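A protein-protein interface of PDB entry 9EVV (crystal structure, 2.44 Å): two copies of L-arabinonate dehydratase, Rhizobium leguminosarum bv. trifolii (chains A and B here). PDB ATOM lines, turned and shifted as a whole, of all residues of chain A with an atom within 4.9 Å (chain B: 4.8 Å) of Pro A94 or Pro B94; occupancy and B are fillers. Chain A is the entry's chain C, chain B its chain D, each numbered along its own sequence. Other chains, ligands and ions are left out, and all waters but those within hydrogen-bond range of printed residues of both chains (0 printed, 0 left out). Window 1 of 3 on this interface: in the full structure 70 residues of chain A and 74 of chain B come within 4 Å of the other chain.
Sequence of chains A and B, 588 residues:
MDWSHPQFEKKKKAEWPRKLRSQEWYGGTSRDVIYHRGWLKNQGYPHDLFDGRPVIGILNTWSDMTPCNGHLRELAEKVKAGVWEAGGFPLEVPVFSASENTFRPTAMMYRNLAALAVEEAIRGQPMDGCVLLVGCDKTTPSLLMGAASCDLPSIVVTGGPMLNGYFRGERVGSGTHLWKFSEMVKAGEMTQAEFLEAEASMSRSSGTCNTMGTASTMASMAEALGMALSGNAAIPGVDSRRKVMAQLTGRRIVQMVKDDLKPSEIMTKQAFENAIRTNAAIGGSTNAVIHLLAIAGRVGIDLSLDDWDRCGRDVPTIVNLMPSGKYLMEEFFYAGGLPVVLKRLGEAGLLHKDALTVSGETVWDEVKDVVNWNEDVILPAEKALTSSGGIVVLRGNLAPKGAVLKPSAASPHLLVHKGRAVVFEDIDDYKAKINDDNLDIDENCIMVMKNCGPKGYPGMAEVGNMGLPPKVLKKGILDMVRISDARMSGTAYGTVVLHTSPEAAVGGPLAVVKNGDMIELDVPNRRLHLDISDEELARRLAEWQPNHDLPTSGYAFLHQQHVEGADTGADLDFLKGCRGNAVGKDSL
The backbone NH (N) of Trp B62 lies within hydrogen-bond range of the side-chain amide oxygen (OD1) of Asn B60 (2.9 Å). OD1 of Asn A60 sits at hydrogen-bond distance from N of Trp A62, 2.8 Å away. O of Val B93 is in hydrogen-bond range of N of Asn B60 (3.1 Å). ND2 of Asn A60 sits at hydrogen-bond distance from OE2 of Glu A92 (2.8 Å). ND2 of Asn B60 is in hydrogen-bond range of OE2 of Glu B92, 2.9 Å away.
Glu B92 touches Trp A62. Trp A62 touches Pro B94. Glu B92 touches Ser A63. OG of Ser A63 touches CG2 of Val B93 (3.8 Å). Trp B62 touches Glu A92. Glu A92 touches Ser B63 (O to OG, 3.8 Å). Pro A94 touches Trp B62. Pro A94 touches Pro B94 (CB to CB, 3.5 Å).
Of chain B, only Trp B62 (3.7 Å) and Pro B94 (3.5 Å) come within 4 Å of Pro A94. Of the printed residues of chain A, Pro B94 touches Trp A62 (3.8 Å) and Pro A94 (3.5 Å). Of the printed residues of chain B, Ser A63 touches Glu B92 and Val B93. Printed residues of chain A within 4 Å of Ser B63: Glu A92. Of the printed residues of chain A, Trp B62 touches Glu A92 and Pro A94. Of the printed residues of chain A, Glu B92 touches Trp A62 (3.7 Å) and Ser A63 (3.6 Å). Printed residues of chain A within 4 Å of Val B93: Ser A63 (3.8 Å). Phe A96 touches none of the printed residues of chain B. Val A95 touches none of the printed residues of chain B. The nearest residue of chain B that does not touch Pro A94 is Ser B63 (4.1 Å). The nearest printed residue of chain A that does not touch Pro B94 is Ser A63 (4.002 Å). The nearest printed residue of chain A that does not touch Val B93 is Trp A62 (5.5 Å).
Of the 8 printed residues of chain B, 5 touch a printed residue of chain A. Printed residues of chain A that touch a printed residue of chain B: Trp A62, Ser A63, Glu A92 and Pro A94. Hydrophobic or aromatic side chains of chain A within 4 Å of the printed part of chain B: Trp A62 and Pro A94. Among the printed residues, 8 pairs touch across the chains. Among the printed residues, no Asp or Glu carboxylate lies within 4 Å of a Lys or Arg side-chain nitrogen of the other chain.
Trp A62 touches Glu B92, and with the chains exchanged Glu A92 touches Trp B62. Trp A62 touches Pro B94, and with the chains exchanged Pro A94 touches Trp B62. Ser A63 touches Val B93, but with the chains exchanged Val A93 does not touch Ser B63 (4.1 Å). Pro B94 touches its own counterpart, Pro A94. Positions printed for both chains: 60, 62, 63, 92, 93, 94, 95 and 96. Of the 8 pairs that touch across the chains among the printed residues, 7 have their exchanged pair printed and touching as well.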
ATOM      1  N   ASN A  60     -12.091  32.048  13.405  1.00  0.00           N
ATOM      2  CA  ASN A  60     -12.142  32.684  14.715  1.00  0.00           C
ATOM      3  C   ASN A  60     -12.271  31.621  15.791  1.00  0.00           C
ATOM      4  O   ASN A  60     -13.143  30.752  15.700  1.00  0.00           O
ATOM      5  CB  ASN A  60     -13.323  33.667  14.787  1.00  0.00           C
ATOM      6  CG  ASN A  60     -13.225  34.639  15.950  1.00  0.00           C
ATOM      7  OD1 ASN A  60     -12.557  34.371  16.940  1.00  0.00           O
ATOM      8  ND2 ASN A  60     -13.919  35.769  15.840  1.00  0.00           N
ATOM      9  N   TRP A  62     -12.809  32.536  18.984  1.00  0.00           N
ATOM     10  CA  TRP A  62     -13.525  33.136  20.098  1.00  0.00           C
ATOM     11  C   TRP A  62     -14.562  32.163  20.661  1.00  0.00           C
ATOM     12  O   TRP A  62     -15.219  31.423  19.927  1.00  0.00           O
ATOM     13  CB  TRP A  62     -14.209  34.446  19.658  1.00  0.00           C
ATOM     14  CG  TRP A  62     -15.111  34.935  20.737  1.00  0.00           C
ATOM     15  CD1 TRP A  62     -14.774  35.757  21.776  1.00  0.00           C
ATOM     16  CD2 TRP A  62     -16.482  34.556  20.950  1.00  0.00           C
ATOM     17  NE1 TRP A  62     -15.851  35.931  22.610  1.00  0.00           N
ATOM     18  CE2 TRP A  62     -16.912  35.201  22.131  1.00  0.00           C
ATOM     19  CE3 TRP A  62     -17.391  33.757  20.245  1.00  0.00           C
ATOM     20  CZ2 TRP A  62     -18.221  35.074  22.622  1.00  0.00           C
ATOM     21  CZ3 TRP A  62     -18.687  33.632  20.731  1.00  0.00           C
ATOM     22  CH2 TRP A  62     -19.089  34.291  21.906  1.00  0.00           C
ATOM     23  N   SER A  63     -14.729  32.192  21.971  1.00  0.00           N
ATOM     24  CA  SER A  63     -15.779  31.419  22.609  1.00  0.00           C
ATOM     25  C   SER A  63     -15.889  31.901  24.045  1.00  0.00           C
ATOM     26  O   SER A  63     -14.889  32.282  24.648  1.00  0.00           O
ATOM     27  CB  SER A  63     -15.468  29.924  22.564  1.00  0.00           C
ATOM     28  OG  SER A  63     -16.232  29.242  23.541  1.00  0.00           O
ATOM     29  N   GLU A  92     -16.602  35.804   8.262  1.00  0.00           N
ATOM     30  CA  GLU A  92     -16.143  35.262   9.528  1.00  0.00           C
ATOM     31  C   GLU A  92     -16.724  33.861   9.713  1.00  0.00           C
ATOM     32  O   GLU A  92     -17.938  33.663   9.577  1.00  0.00           O
ATOM     33  CB  GLU A  92     -16.554  36.186  10.678  1.00  0.00           C
ATOM     34  CG  GLU A  92     -15.839  35.889  11.963  1.00  0.00           C
ATOM     35  CD  GLU A  92     -16.453  36.549  13.192  1.00  0.00           C
ATOM     36  OE1 GLU A  92     -17.108  37.624  13.076  1.00  0.00           O
ATOM     37  OE2 GLU A  92     -16.267  35.961  14.291  1.00  0.00           O
ATOM     38  N   VAL A  93     -15.854  32.897  10.012  1.00  0.00           N
ATOM     39  CA  VAL A  93     -16.198  31.488  10.192  1.00  0.00           C
ATOM     40  C   VAL A  93     -15.670  31.016  11.543  1.00  0.00           C
ATOM     41  O   VAL A  93     -14.458  30.809  11.678  1.00  0.00           O
ATOM     42  CB  VAL A  93     -15.601  30.639   9.062  1.00  0.00           C
ATOM     43  CG1 VAL A  93     -15.943  29.138   9.244  1.00  0.00           C
ATOM     44  CG2 VAL A  93     -16.075  31.176   7.746  1.00  0.00           C
ATOM     45  N   PRO A  94     -16.512  30.849  12.564  1.00  0.00           N
ATOM     46  CA  PRO A  94     -16.041  30.215  13.800  1.00  0.00           C
ATOM     47  C   PRO A  94     -15.535  28.809  13.524  1.00  0.00           C
ATOM     48  O   PRO A  94     -16.064  28.099  12.662  1.00  0.00           O
ATOM     49  CB  PRO A  94     -17.288  30.186  14.686  1.00  0.00           C
ATOM     50  CG  PRO A  94     -18.139  31.328  14.156  1.00  0.00           C
ATOM     51  CD  PRO A  94     -17.917  31.269  12.665  1.00  0.00           C
ATOM     52  N   VAL A  95     -14.503  28.409  14.284  1.00  0.00           N
ATOM     53  CA  VAL A  95     -13.926  27.067  14.200  1.00  0.00           C
ATOM     54  C   VAL A  95     -13.607  26.554  15.606  1.00  0.00           C
ATOM     55  O   VAL A  95     -13.583  27.309  16.579  1.00  0.00           O
ATOM     56  CB  VAL A  95     -12.678  27.049  13.295  1.00  0.00           C
ATOM     57  CG1 VAL A  95     -13.047  27.544  11.888  1.00  0.00           C
ATOM     58  CG2 VAL A  95     -11.574  27.926  13.879  1.00  0.00           C
ATOM     59  N   PHE A  96     -13.351  25.245  15.704  1.00  0.00           N
ATOM     60  CA  PHE A  96     -13.185  24.571  17.000  1.00  0.00           C
ATOM     61  C   PHE A  96     -12.113  25.249  17.838  1.00  0.00           C
ATOM     62  O   PHE A  96     -10.975  25.403  17.392  1.00  0.00           O
ATOM     63  CB  PHE A  96     -12.822  23.091  16.782  1.00  0.00           C
ATOM     64  CG  PHE A  96     -13.023  22.229  17.998  1.00  0.00           C
ATOM     65  CD1 PHE A  96     -12.111  22.261  19.045  1.00  0.00           C
ATOM     66  CD2 PHE A  96     -14.132  21.398  18.103  1.00  0.00           C
ATOM     67  CE1 PHE A  96     -12.309  21.469  20.179  1.00  0.00           C
ATOM     68  CE2 PHE A  96     -14.341  20.621  19.228  1.00  0.00           C
ATOM     69  CZ  PHE A  96     -13.427  20.644  20.262  1.00  0.00           C
ATOM     70  N   ASN B  60     -23.790  27.367  19.068  1.00  0.00           N
ATOM     71  CA  ASN B  60     -24.250  28.299  18.052  1.00  0.00           C
ATOM     72  C   ASN B  60     -23.610  27.976  16.717  1.00  0.00           C
ATOM     73  O   ASN B  60     -22.388  28.075  16.578  1.00  0.00           O
ATOM     74  CB  ASN B  60     -23.924  29.739  18.437  1.00  0.00           C
ATOM     75  CG  ASN B  60     -24.643  30.734  17.559  1.00  0.00           C
ATOM     76  OD1 ASN B  60     -25.288  30.356  16.569  1.00  0.00           O
ATOM     77  ND2 ASN B  60     -24.553  32.006  17.914  1.00  0.00           N
ATOM     78  N   TRP B  62     -24.024  29.697  14.027  1.00  0.00           N
ATOM     79  CA  TRP B  62     -23.885  30.920  13.246  1.00  0.00           C
ATOM     80  C   TRP B  62     -22.584  30.896  12.431  1.00  0.00           C
ATOM     81  O   TRP B  62     -21.623  30.193  12.760  1.00  0.00           O
ATOM     82  CB  TRP B  62     -23.907  32.163  14.159  1.00  0.00           C
ATOM     83  CG  TRP B  62     -23.545  33.386  13.368  1.00  0.00           C
ATOM     84  CD1 TRP B  62     -24.379  34.092  12.557  1.00  0.00           C
ATOM     85  CD2 TRP B  62     -22.246  33.985  13.222  1.00  0.00           C
ATOM     86  NE1 TRP B  62     -23.699  35.101  11.936  1.00  0.00           N
ATOM     87  CE2 TRP B  62     -22.388  35.068  12.329  1.00  0.00           C
ATOM     88  CE3 TRP B  62     -20.986  33.730  13.770  1.00  0.00           C
ATOM     89  CZ2 TRP B  62     -21.317  35.897  11.972  1.00  0.00           C
ATOM     90  CZ3 TRP B  62     -19.922  34.570  13.421  1.00  0.00           C
ATOM     91  CH2 TRP B  62     -20.097  35.631  12.525  1.00  0.00           C
ATOM     92  N   SER B  63     -22.552  31.702  11.365  1.00  0.00           N
ATOM     93  CA  SER B  63     -21.382  31.805  10.501  1.00  0.00           C
ATOM     94  C   SER B  63     -21.672  32.689   9.290  1.00  0.00           C
ATOM     95  O   SER B  63     -22.703  32.526   8.633  1.00  0.00           O
ATOM     96  CB  SER B  63     -20.946  30.403  10.061  1.00  0.00           C
ATOM     97  OG  SER B  63     -19.962  30.456   9.053  1.00  0.00           O
ATOM     98  N   GLU B  92     -21.742  31.237  25.442  1.00  0.00           N
ATOM     99  CA  GLU B  92     -21.915  30.918  24.027  1.00  0.00           C
ATOM    100  C   GLU B  92     -20.699  30.175  23.483  1.00  0.00           C
ATOM    101  O   GLU B  92     -19.552  30.653  23.604  1.00  0.00           O
ATOM    102  CB  GLU B  92     -22.115  32.187  23.212  1.00  0.00           C
ATOM    103  CG  GLU B  92     -22.324  31.886  21.735  1.00  0.00           C
ATOM    104  CD  GLU B  92     -22.524  33.154  20.894  1.00  0.00           C
ATOM    105  OE1 GLU B  92     -22.766  34.232  21.496  1.00  0.00           O
ATOM    106  OE2 GLU B  92     -22.432  33.065  19.635  1.00  0.00           O
ATOM    107  N   VAL B  93     -20.953  29.035  22.844  1.00  0.00           N
ATOM    108  CA  VAL B  93     -19.892  28.195  22.296  1.00  0.00           C
ATOM    109  C   VAL B  93     -20.198  27.927  20.834  1.00  0.00           C
ATOM    110  O   VAL B  93     -21.119  27.157  20.538  1.00  0.00           O
ATOM    111  CB  VAL B  93     -19.755  26.880  23.080  1.00  0.00           C
ATOM    112  CG1 VAL B  93     -18.831  25.889  22.335  1.00  0.00           C
ATOM    113  CG2 VAL B  93     -19.291  27.152  24.530  1.00  0.00           C
ATOM    114  N   PRO B  94     -19.489  28.543  19.895  1.00  0.00           N
ATOM    115  CA  PRO B  94     -19.718  28.220  18.486  1.00  0.00           C
ATOM    116  C   PRO B  94     -19.358  26.769  18.209  1.00  0.00           C
ATOM    117  O   PRO B  94     -18.493  26.174  18.865  1.00  0.00           O
ATOM    118  CB  PRO B  94     -18.786  29.185  17.743  1.00  0.00           C
ATOM    119  CG  PRO B  94     -18.604  30.332  18.682  1.00  0.00           C
ATOM    120  CD  PRO B  94     -18.577  29.688  20.055  1.00  0.00           C
ATOM    121  N   VAL B  95     -20.032  26.191  17.216  1.00  0.00           N
ATOM    122  CA  VAL B  95     -19.745  24.825  16.820  1.00  0.00           C
ATOM    123  C   VAL B  95     -19.857  24.707  15.313  1.00  0.00           C
ATOM    124  O   VAL B  95     -20.472  25.535  14.637  1.00  0.00           O
ATOM    125  CB  VAL B  95     -20.691  23.827  17.505  1.00  0.00           C
ATOM    126  CG1 VAL B  95     -20.396  23.761  18.985  1.00  0.00           C
ATOM    127  CG2 VAL B  95     -22.146  24.236  17.263  1.00  0.00           C
ATOM    128  N   PHE B  96     -19.266  23.641  14.800  1.00  0.00           N
ATOM    129  CA  PHE B  96     -19.282  23.338  13.378  1.00  0.00           C
ATOM    130  C   PHE B  96     -20.643  23.623  12.769  1.00  0.00           C
ATOM    131  O   PHE B  96     -21.667  23.097  13.227  1.00  0.00           O
ATOM    132  CB  PHE B  96     -18.905  21.866  13.165  1.00  0.00           C
ATOM    133  CG  PHE B  96     -18.286  21.596  11.825  1.00  0.00           C
ATOM    134  CD1 PHE B  96     -19.093  21.349  10.710  1.00  0.00           C
ATOM    135  CD2 PHE B  96     -16.899  21.605  11.672  1.00  0.00           C
ATOM    136  CE1 PHE B  96     -18.532  21.120   9.470  1.00  0.00           C
ATOM    137  CE2 PHE B  96     -16.321  21.368  10.432  1.00  0.00           C
ATOM    138  CZ  PHE B  96     -17.137  21.122   9.328  1.00  0.00           C
